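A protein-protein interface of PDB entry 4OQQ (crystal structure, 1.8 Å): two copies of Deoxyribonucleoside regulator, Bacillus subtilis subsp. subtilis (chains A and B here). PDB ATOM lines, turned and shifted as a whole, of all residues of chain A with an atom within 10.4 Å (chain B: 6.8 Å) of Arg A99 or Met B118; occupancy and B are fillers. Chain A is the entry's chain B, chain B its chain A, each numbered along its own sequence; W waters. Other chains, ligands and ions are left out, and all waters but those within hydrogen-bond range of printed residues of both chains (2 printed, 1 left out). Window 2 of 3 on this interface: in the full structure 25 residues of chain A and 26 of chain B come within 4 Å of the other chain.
Among the printed residues, merely in contact across the chains: His A97 with Arg B120 (3.3 Å), Ser A96 with Arg B120 (3.4 Å), Asn A101 with Gln B109 (3.5 Å), His A97 with Met B118 (3.6 Å), Ser A96 with Pro B119 (3.7 Å), Ser A98 with Met B118 (3.7 Å) and Ile A95 with Tyr B121 (3.8 Å).
Water W1 bridges O of Pro B119 (2.7 Å) and O of Ser A98 (3.0 Å). Water W2 lies within hydrogen-bond range of the side-chain hydroxyl of Ser A96 (3.1 Å) and the guanidinium group of Arg B120 (3.2 Å).
Of chain B, only Met B118 comes within 4 Å of Arg A99. Of the printed residues of chain A, Met B118 touches His A97 (3.6 Å), Ser A98 (3.7 Å) and Arg A99 (3.1 Å). Val B88 touches none of the printed residues of chain A. No residue of chain A comes within 4 Å of Ala B112. No residue of chain A comes within 4 Å of Thr B117. Of the printed residues of chain B, His A97 touches Met B118, Pro B119 and Arg B120. Of the printed residues of chain B, Ser A96 touches Pro B119, Arg B120 and Tyr B121. Of the printed residues of chain A, Arg B120 touches Ser A96 and His A97. Of the printed residues of chain A, Gln B109 touches Asn A101 (3.5 Å). Of the printed residues of chain B, Asn A101 touches Gln B109 (3.5 Å). The nearest residue of chain B that does not touch Arg A99 is Arg B120 (4.4 Å).
Printed residues of chain A that touch a printed residue of chain B: Ile A95, Ser A96, His A97, Ser A98, Arg A99 and Asn A101. Hydrophobic or aromatic side chains of chain A that line the printed part of chain B: His A97. Along chain B the printed residues that touch a printed residue of chain A span positions 109 to 121. Among the printed residues, no Asp or Glu carboxylate lies within 4 Å of a Lys or Arg side-chain nitrogen of the other chain.
O of Arg A99 sits close to SD of Met B118 (3.1 Å). A ring nitrogen (ND1) of His A97 is in hydrogen-bond range of the backbone carbonyl oxygen (O) of Pro B119. OG of Ser A96 sits at hydrogen-bond distance from O of Tyr B121 (2.7 Å).
No position is printed for both chains. Of the 10 pairs that touch across the chains among the printed residues, none has its exchanged pair printed and touching as well.
OG of Ser A98 lies within hydrogen-bond range of O of Val A100, at 2.6 Å. The backbone NH of Tyr A103 lies within hydrogen-bond range of the side-chain amide oxygen of Asn A101, at 2.8 Å. The side-chain carboxylate (OE1) of Glu B87 lies within salt-bridge range of the guanidinium group (NE) of Arg B120. NE2 of His A97 lies within hydrogen-bond range of NE of Arg A99, 3.3 Å away. The side-chain amide oxygen (OE1) of Gln B109 lies close to the side-chain carboxylate (OE2) of Glu B113 (3.1 Å). N of Arg B120 lies within hydrogen-bond range of O of Val B88, 2.9 Å away.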
ATOM      1  N   ILE A  95      37.361 -19.607  -0.566  1.00  0.00           N
ATOM      2  CA  ILE A  95      36.165 -19.653  -1.365  1.00  0.00           C
ATOM      3  C   ILE A  95      35.230 -18.566  -0.865  1.00  0.00           C
ATOM      4  O   ILE A  95      35.402 -17.994   0.216  1.00  0.00           O
ATOM      5  CB  ILE A  95      35.443 -21.031  -1.321  1.00  0.00           C
ATOM      6  CG1 ILE A  95      34.996 -21.331   0.132  1.00  0.00           C
ATOM      7  CG2 ILE A  95      36.362 -22.106  -1.911  1.00  0.00           C
ATOM      8  CD1 ILE A  95      34.017 -22.464   0.220  1.00  0.00           C
ATOM      9  N   SER A  96      34.222 -18.260  -1.649  1.00  0.00           N
ATOM     10  CA  SER A  96      33.384 -17.169  -1.220  1.00  0.00           C
ATOM     11  C   SER A  96      32.138 -17.665  -0.538  1.00  0.00           C
ATOM     12  O   SER A  96      31.602 -16.954   0.302  1.00  0.00           O
ATOM     13  CB  SER A  96      33.037 -16.199  -2.334  1.00  0.00           C
ATOM     14  OG  SER A  96      32.059 -15.289  -1.834  1.00  0.00           O
ATOM     15  N   HIS A  97      31.690 -18.877  -0.854  1.00  0.00           N
ATOM     16  CA  HIS A  97      30.564 -19.485  -0.186  1.00  0.00           C
ATOM     17  C   HIS A  97      30.642 -21.017  -0.329  1.00  0.00           C
ATOM     18  O   HIS A  97      31.164 -21.503  -1.325  1.00  0.00           O
ATOM     19  CB  HIS A  97      29.269 -19.013  -0.842  1.00  0.00           C
ATOM     20  CG  HIS A  97      28.033 -19.627  -0.255  1.00  0.00           C
ATOM     21  ND1 HIS A  97      27.403 -19.121   0.862  1.00  0.00           N
ATOM     22  CD2 HIS A  97      27.284 -20.690  -0.653  1.00  0.00           C
ATOM     23  CE1 HIS A  97      26.330 -19.846   1.139  1.00  0.00           C
ATOM     24  NE2 HIS A  97      26.238 -20.812   0.243  1.00  0.00           N
ATOM     25  N   SER A  98      30.173 -21.742   0.689  1.00  0.00           N
ATOM     26  CA  SER A  98      29.712 -23.146   0.545  1.00  0.00           C
ATOM     27  C   SER A  98      28.726 -23.431   1.668  1.00  0.00           C
ATOM     28  O   SER A  98      28.749 -22.769   2.700  1.00  0.00           O
ATOM     29  CB  SER A  98      30.867 -24.145   0.603  1.00  0.00           C
ATOM     30  OG  SER A  98      31.615 -23.977   1.800  1.00  0.00           O
ATOM     31  N   ARG A  99      27.863 -24.418   1.464  1.00  0.00           N
ATOM     32  CA  ARG A  99      26.870 -24.777   2.463  1.00  0.00           C
ATOM     33  C   ARG A  99      27.495 -25.486   3.664  1.00  0.00           C
ATOM     34  O   ARG A  99      26.874 -25.545   4.716  1.00  0.00           O
ATOM     35  CB  ARG A  99      25.752 -25.636   1.862  1.00  0.00           C
ATOM     36  CG  ARG A  99      24.961 -24.952   0.754  1.00  0.00           C
ATOM     37  CD  ARG A  99      24.018 -23.857   1.260  1.00  0.00           C
ATOM     38  NE  ARG A  99      23.702 -22.893   0.198  1.00  0.00           N
ATOM     39  CZ  ARG A  99      22.724 -21.988   0.234  1.00  0.00           C
ATOM     40  NH1 ARG A  99      21.914 -21.888   1.285  1.00  0.00           N
ATOM     41  NH2 ARG A  99      22.550 -21.174  -0.804  1.00  0.00           N
ATOM     42  N   VAL A 100      28.700 -26.031   3.515  1.00  0.00           N
ATOM     43  CA  VAL A 100      29.471 -26.549   4.654  1.00  0.00           C
ATOM     44  C   VAL A 100      30.628 -25.587   5.003  1.00  0.00           C
ATOM     45  O   VAL A 100      31.346 -25.070   4.125  1.00  0.00           O
ATOM     46  CB  VAL A 100      30.000 -27.992   4.402  1.00  0.00           C
ATOM     47  CG1 VAL A 100      31.252 -28.006   3.516  1.00  0.00           C
ATOM     48  CG2 VAL A 100      30.273 -28.699   5.723  1.00  0.00           C
ATOM     49  N   ASN A 101      30.789 -25.318   6.289  1.00  0.00           N
ATOM     50  CA  ASN A 101      31.858 -24.444   6.729  1.00  0.00           C
ATOM     51  C   ASN A 101      33.204 -25.130   6.432  1.00  0.00           C
ATOM     52  O   ASN A 101      33.379 -26.297   6.786  1.00  0.00           O
ATOM     53  CB  ASN A 101      31.673 -24.189   8.222  1.00  0.00           C
ATOM     54  CG  ASN A 101      32.606 -23.135   8.768  1.00  0.00           C
ATOM     55  OD1 ASN A 101      33.631 -22.801   8.167  1.00  0.00           O
ATOM     56  ND2 ASN A 101      32.249 -22.601   9.945  1.00  0.00           N
ATOM     57  N   THR A 102      34.144 -24.422   5.801  1.00  0.00           N
ATOM     58  CA  THR A 102      35.477 -24.994   5.507  1.00  0.00           C
ATOM     59  C   THR A 102      36.414 -25.001   6.705  1.00  0.00           C
ATOM     60  O   THR A 102      37.493 -25.682   6.712  1.00  0.00           O
ATOM     61  CB  THR A 102      36.193 -24.215   4.404  1.00  0.00           C
ATOM     62  OG1 THR A 102      36.598 -22.924   4.902  1.00  0.00           O
ATOM     63  CG2 THR A 102      35.302 -24.053   3.158  1.00  0.00           C
ATOM     64  N   TYR A 103      36.036 -24.200   7.705  1.00  0.00           N
ATOM     65  CA  TYR A 103      36.788 -24.049   8.942  1.00  0.00           C
ATOM     66  C   TYR A 103      38.205 -23.601   8.706  1.00  0.00           C
ATOM     67  O   TYR A 103      39.091 -23.776   9.549  1.00  0.00           O
ATOM     68  CB  TYR A 103      36.738 -25.334   9.780  1.00  0.00           C
ATOM     69  CG  TYR A 103      35.351 -25.626  10.309  1.00  0.00           C
ATOM     70  CD1 TYR A 103      34.816 -24.874  11.353  1.00  0.00           C
ATOM     71  CD2 TYR A 103      34.568 -26.652   9.765  1.00  0.00           C
ATOM     72  CE1 TYR A 103      33.541 -25.133  11.847  1.00  0.00           C
ATOM     73  CE2 TYR A 103      33.287 -26.915  10.253  1.00  0.00           C
ATOM     74  CZ  TYR A 103      32.785 -26.147  11.291  1.00  0.00           C
ATOM     75  OH  TYR A 103      31.529 -26.377  11.783  1.00  0.00           O
ATOM     76  N   GLU A 106      39.523 -21.071  11.463  1.00  0.00           N
ATOM     77  CA  GLU A 106      39.708 -21.800  12.723  1.00  0.00           C
ATOM     78  C   GLU A 106      40.912 -22.713  12.663  1.00  0.00           C
ATOM     79  O   GLU A 106      41.645 -22.859  13.636  1.00  0.00           O
ATOM     80  CB  GLU A 106      38.473 -22.641  12.997  1.00  0.00           C
ATOM     81  CG  GLU A 106      37.270 -21.834  13.436  1.00  0.00           C
ATOM     82  CD  GLU A 106      36.431 -21.273  12.303  1.00  0.00           C
ATOM     83  OE1 GLU A 106      36.848 -21.305  11.102  1.00  0.00           O
ATOM     84  OE2 GLU A 106      35.333 -20.773  12.630  1.00  0.00           O
ATOM     85  N   GLU A 166      31.295 -34.921  -6.252  1.00  0.00           N
ATOM     86  CA  GLU A 166      31.032 -34.226  -4.968  1.00  0.00           C
ATOM     87  C   GLU A 166      31.934 -33.043  -4.742  1.00  0.00           C
ATOM     88  O   GLU A 166      31.530 -32.096  -4.074  1.00  0.00           O
ATOM     89  CB  GLU A 166      31.296 -35.125  -3.739  1.00  0.00           C
ATOM     90  CG  GLU A 166      30.888 -36.588  -3.796  1.00  0.00           C
ATOM     91  CD  GLU A 166      29.410 -36.766  -3.969  1.00  0.00           C
ATOM     92  OE1 GLU A 166      28.645 -35.845  -3.591  1.00  0.00           O
ATOM     93  OE2 GLU A 166      29.019 -37.826  -4.473  1.00  0.00           O
ATOM     94  N   LEU A 168      34.296 -30.111  -3.901  1.00  0.00           N
ATOM     95  CA  LEU A 168      33.940 -28.715  -3.721  1.00  0.00           C
ATOM     96  C   LEU A 168      34.215 -27.875  -4.959  1.00  0.00           C
ATOM     97  O   LEU A 168      33.352 -27.104  -5.426  1.00  0.00           O
ATOM     98  CB  LEU A 168      34.700 -28.159  -2.528  1.00  0.00           C
ATOM     99  CG  LEU A 168      34.356 -26.739  -2.135  1.00  0.00           C
ATOM    100  CD1 LEU A 168      32.851 -26.539  -1.953  1.00  0.00           C
ATOM    101  CD2 LEU A 168      35.110 -26.423  -0.870  1.00  0.00           C
ATOM    102  N   ARG A 171      31.918 -27.345  -7.923  1.00  0.00           N
ATOM    103  CA  ARG A 171      30.590 -26.919  -7.564  1.00  0.00           C
ATOM    104  C   ARG A 171      30.571 -25.466  -7.209  1.00  0.00           C
ATOM    105  O   ARG A 171      29.653 -25.005  -6.566  1.00  0.00           O
ATOM    106  CB  ARG A 171      30.127 -27.773  -6.396  1.00  0.00           C
ATOM    107  CG  ARG A 171      30.068 -29.254  -6.774  1.00  0.00           C
ATOM    108  CD  ARG A 171      29.755 -30.137  -5.594  1.00  0.00           C
ATOM    109  NE  ARG A 171      28.430 -29.852  -5.067  1.00  0.00           N
ATOM    110  CZ  ARG A 171      27.965 -30.354  -3.934  1.00  0.00           C
ATOM    111  NH1 ARG A 171      28.736 -31.167  -3.214  1.00  0.00           N
ATOM    112  NH2 ARG A 171      26.739 -30.043  -3.520  1.00  0.00           N
ATOM    113  N   LEU A 172      31.550 -24.715  -7.674  1.00  0.00           N
ATOM    114  CA  LEU A 172      31.657 -23.331  -7.246  1.00  0.00           C
ATOM    115  C   LEU A 172      31.635 -22.310  -8.395  1.00  0.00           C
ATOM    116  O   LEU A 172      31.875 -21.121  -8.192  1.00  0.00           O
ATOM    117  CB  LEU A 172      32.921 -23.175  -6.408  1.00  0.00           C
ATOM    118  CG  LEU A 172      32.856 -23.683  -4.974  1.00  0.00           C
ATOM    119  CD1 LEU A 172      34.228 -23.612  -4.327  1.00  0.00           C
ATOM    120  CD2 LEU A 172      31.895 -22.823  -4.177  1.00  0.00           C
ATOM    121  N   VAL B  86      17.343 -15.599   3.521  1.00  0.00           N
ATOM    122  CA  VAL B  86      18.260 -14.535   3.937  1.00  0.00           C
ATOM    123  C   VAL B  86      19.695 -14.858   3.511  1.00  0.00           C
ATOM    124  O   VAL B  86      20.175 -15.965   3.690  1.00  0.00           O
ATOM    125  CB  VAL B  86      18.177 -14.259   5.455  1.00  0.00           C
ATOM    126  CG1 VAL B  86      19.259 -13.296   5.940  1.00  0.00           C
ATOM    127  CG2 VAL B  86      16.839 -13.622   5.746  1.00  0.00           C
ATOM    128  N   GLU B  87      20.376 -13.869   2.961  1.00  0.00           N
ATOM    129  CA  GLU B  87      21.813 -13.977   2.748  1.00  0.00           C
ATOM    130  C   GLU B  87      22.561 -12.938   3.591  1.00  0.00           C
ATOM    131  O   GLU B  87      22.034 -11.843   3.867  1.00  0.00           O
ATOM    132  CB  GLU B  87      22.114 -13.748   1.298  1.00  0.00           C
ATOM    133  CG  GLU B  87      21.488 -14.736   0.334  1.00  0.00           C
ATOM    134  CD  GLU B  87      22.451 -15.812  -0.140  1.00  0.00           C
ATOM    135  OE1 GLU B  87      23.568 -15.908   0.410  1.00  0.00           O
ATOM    136  OE2 GLU B  87      22.087 -16.556  -1.082  1.00  0.00           O
ATOM    137  N   VAL B  88      23.770 -13.308   4.014  1.00  0.00           N
ATOM    138  CA  VAL B  88      24.606 -12.491   4.843  1.00  0.00           C
ATOM    139  C   VAL B  88      25.957 -12.377   4.122  1.00  0.00           C
ATOM    140  O   VAL B  88      26.632 -13.385   3.934  1.00  0.00           O
ATOM    141  CB  VAL B  88      24.853 -13.130   6.199  1.00  0.00           C
ATOM    142  CG1 VAL B  88      25.885 -12.325   6.984  1.00  0.00           C
ATOM    143  CG2 VAL B  88      23.543 -13.188   6.984  1.00  0.00           C
ATOM    144  N   VAL B  89      26.354 -11.164   3.794  1.00  0.00           N
ATOM    145  CA  VAL B  89      27.532 -10.924   2.951  1.00  0.00           C
ATOM    146  C   VAL B  89      28.509  -9.988   3.625  1.00  0.00           C
ATOM    147  O   VAL B  89      28.131  -9.036   4.332  1.00  0.00           O
ATOM    148  CB  VAL B  89      27.081 -10.402   1.579  1.00  0.00           C
ATOM    149  CG1 VAL B  89      26.449  -9.012   1.704  1.00  0.00           C
ATOM    150  CG2 VAL B  89      28.232 -10.387   0.587  1.00  0.00           C
ATOM    151  N   ILE B 108      30.928 -13.114  10.866  1.00  0.00           N
ATOM    152  CA  ILE B 108      29.976 -13.347   9.783  1.00  0.00           C
ATOM    153  C   ILE B 108      29.328 -14.717   9.896  1.00  0.00           C
ATOM    154  O   ILE B 108      28.148 -14.872   9.570  1.00  0.00           O
ATOM    155  CB  ILE B 108      30.564 -13.100   8.371  1.00  0.00           C
ATOM    156  CG1 ILE B 108      29.422 -13.105   7.358  1.00  0.00           C
ATOM    157  CG2 ILE B 108      31.617 -14.125   8.001  1.00  0.00           C
ATOM    158  CD1 ILE B 108      29.780 -12.546   5.998  1.00  0.00           C
ATOM    159  N   GLN B 109      30.080 -15.702  10.372  1.00  0.00           N
ATOM    160  CA  GLN B 109      29.497 -17.013  10.721  1.00  0.00           C
ATOM    161  C   GLN B 109      28.322 -16.897  11.705  1.00  0.00           C
ATOM    162  O   GLN B 109      27.237 -17.471  11.472  1.00  0.00           O
ATOM    163  CB  GLN B 109      30.576 -17.952  11.309  1.00  0.00           C
ATOM    164  CG  GLN B 109      30.202 -19.429  11.401  1.00  0.00           C
ATOM    165  CD  GLN B 109      29.707 -20.033  10.087  1.00  0.00           C
ATOM    166  OE1 GLN B 109      28.710 -20.755  10.061  1.00  0.00           O
ATOM    167  NE2 GLN B 109      30.401 -19.745   8.991  1.00  0.00           N
ATOM    168  N   ALA B 112      25.435 -15.298  10.154  1.00  0.00           N
ATOM    169  CA  ALA B 112      24.836 -16.147   9.144  1.00  0.00           C
ATOM    170  C   ALA B 112      23.988 -17.213   9.796  1.00  0.00           C
ATOM    171  O   ALA B 112      22.860 -17.454   9.384  1.00  0.00           O
ATOM    172  CB  ALA B 112      25.904 -16.787   8.296  1.00  0.00           C
ATOM    173  N   GLU B 113      24.536 -17.810  10.839  1.00  0.00           N
ATOM    174  CA  GLU B 113      23.862 -18.883  11.539  1.00  0.00           C
ATOM    175  C   GLU B 113      22.582 -18.385  12.174  1.00  0.00           C
ATOM    176  O   GLU B 113      21.550 -19.055  12.095  1.00  0.00           O
ATOM    177  CB  GLU B 113      24.796 -19.523  12.564  1.00  0.00           C
ATOM    178  CG  GLU B 113      25.780 -20.468  11.900  1.00  0.00           C
ATOM    179  CD  GLU B 113      26.866 -20.988  12.822  1.00  0.00           C
ATOM    180  OE1 GLU B 113      27.246 -20.313  13.803  1.00  0.00           O
ATOM    181  OE2 GLU B 113      27.373 -22.082  12.536  1.00  0.00           O
ATOM    182  N   PHE B 115      20.633 -16.306  11.126  1.00  0.00           N
ATOM    183  CA  PHE B 115      19.643 -16.137  10.045  1.00  0.00           C
ATOM    184  C   PHE B 115      19.492 -17.330   9.069  1.00  0.00           C
ATOM    185  O   PHE B 115      18.971 -17.187   7.951  1.00  0.00           O
ATOM    186  CB  PHE B 115      19.894 -14.819   9.286  1.00  0.00           C
ATOM    187  CG  PHE B 115      19.899 -13.588  10.168  1.00  0.00           C
ATOM    188  CD1 PHE B 115      18.849 -13.336  11.059  1.00  0.00           C
ATOM    189  CD2 PHE B 115      20.937 -12.658  10.085  1.00  0.00           C
ATOM    190  CE1 PHE B 115      18.852 -12.207  11.869  1.00  0.00           C
ATOM    191  CE2 PHE B 115      20.937 -11.529  10.886  1.00  0.00           C
ATOM    192  CZ  PHE B 115      19.900 -11.298  11.777  1.00  0.00           C
ATOM    193  N   GLN B 116      19.891 -18.518   9.527  1.00  0.00           N
ATOM    194  CA  GLN B 116      19.629 -19.779   8.806  1.00  0.00           C
ATOM    195  C   GLN B 116      20.241 -19.802   7.411  1.00  0.00           C
ATOM    196  O   GLN B 116      19.633 -20.285   6.452  1.00  0.00           O
ATOM    197  CB  GLN B 116      18.118 -20.074   8.734  1.00  0.00           C
ATOM    198  CG  GLN B 116      17.374 -19.751  10.019  1.00  0.00           C
ATOM    199  CD  GLN B 116      17.903 -20.557  11.201  1.00  0.00           C
ATOM    200  OE1 GLN B 116      17.937 -21.794  11.162  1.00  0.00           O
ATOM    201  NE2 GLN B 116      18.341 -19.854  12.254  1.00  0.00           N
ATOM    202  N   THR B 117      21.437 -19.241   7.298  1.00  0.00           N
ATOM    203  CA  THR B 117      22.176 -19.297   6.048  1.00  0.00           C
ATOM    204  C   THR B 117      23.662 -19.467   6.383  1.00  0.00           C
ATOM    205  O   THR B 117      24.018 -19.752   7.547  1.00  0.00           O
ATOM    206  CB  THR B 117      21.879 -18.041   5.195  1.00  0.00           C
ATOM    207  OG1 THR B 117      22.451 -18.180   3.887  1.00  0.00           O
ATOM    208  CG2 THR B 117      22.426 -16.764   5.870  1.00  0.00           C
ATOM    209  N   MET B 118      24.514 -19.299   5.366  1.00  0.00           N
ATOM    210  CA  MET B 118      25.970 -19.450   5.495  1.00  0.00           C
ATOM    211  C   MET B 118      26.606 -18.170   4.938  1.00  0.00           C
ATOM    212  O   MET B 118      26.057 -17.574   4.025  1.00  0.00           O
ATOM    213  CB  MET B 118      26.455 -20.654   4.683  1.00  0.00           C
ATOM    214  CG  MET B 118      25.934 -22.015   5.167  1.00  0.00           C
ATOM    215  SD  MET B 118      27.144 -22.858   6.203  1.00  0.00           S
ATOM    216  CE  MET B 118      26.787 -22.112   7.799  1.00  0.00           C
ATOM    217  N   PRO B 119      27.765 -17.765   5.470  1.00  0.00           N
ATOM    218  CA  PRO B 119      28.454 -16.521   5.045  1.00  0.00           C
ATOM    219  C   PRO B 119      28.790 -16.442   3.584  1.00  0.00           C
ATOM    220  O   PRO B 119      29.145 -17.459   2.966  1.00  0.00           O
ATOM    221  CB  PRO B 119      29.734 -16.523   5.851  1.00  0.00           C
ATOM    222  CG  PRO B 119      29.628 -17.604   6.827  1.00  0.00           C
ATOM    223  CD  PRO B 119      28.573 -18.548   6.408  1.00  0.00           C
ATOM    224  N   ARG B 120      28.686 -15.233   3.031  1.00  0.00           N
ATOM    225  CA  ARG B 120      29.193 -14.943   1.713  1.00  0.00           C
ATOM    226  C   ARG B 120      30.407 -14.080   1.969  1.00  0.00           C
ATOM    227  O   ARG B 120      30.279 -12.902   2.333  1.00  0.00           O
ATOM    228  CB  ARG B 120      28.154 -14.238   0.855  1.00  0.00           C
ATOM    229  CG  ARG B 120      26.887 -15.070   0.593  1.00  0.00           C
ATOM    230  CD  ARG B 120      27.035 -15.907  -0.683  1.00  0.00           C
ATOM    231  NE  ARG B 120      25.777 -16.414  -1.228  1.00  0.00           N
ATOM    232  CZ  ARG B 120      25.689 -17.317  -2.205  1.00  0.00           C
ATOM    233  NH1 ARG B 120      26.775 -17.826  -2.763  1.00  0.00           N
ATOM    234  NH2 ARG B 120      24.495 -17.732  -2.624  1.00  0.00           N
ATOM    235  N   TYR B 121      31.587 -14.688   1.875  1.00  0.00           N
ATOM    236  CA  TYR B 121      32.822 -14.000   2.230  1.00  0.00           C
ATOM    237  C   TYR B 121      33.247 -13.120   1.063  1.00  0.00           C
ATOM    238  O   TYR B 121      32.771 -13.299  -0.076  1.00  0.00           O
ATOM    239  CB  TYR B 121      33.943 -14.976   2.525  1.00  0.00           C
ATOM    240  CG  TYR B 121      33.678 -15.979   3.609  1.00  0.00           C
ATOM    241  CD1 TYR B 121      33.809 -15.637   4.938  1.00  0.00           C
ATOM    242  CD2 TYR B 121      33.335 -17.303   3.291  1.00  0.00           C
ATOM    243  CE1 TYR B 121      33.584 -16.572   5.941  1.00  0.00           C
ATOM    244  CE2 TYR B 121      33.109 -18.234   4.278  1.00  0.00           C
ATOM    245  CZ  TYR B 121      33.238 -17.857   5.599  1.00  0.00           C
ATOM    246  OH  TYR B 121      33.008 -18.792   6.578  1.00  0.00           O
HETATM  247  O   HOH W   1      29.865 -20.032   3.418  1.00  0.00           O
HETATM  248  O   HOH W   2      29.285 -15.832  -3.099  1.00  0.00           O
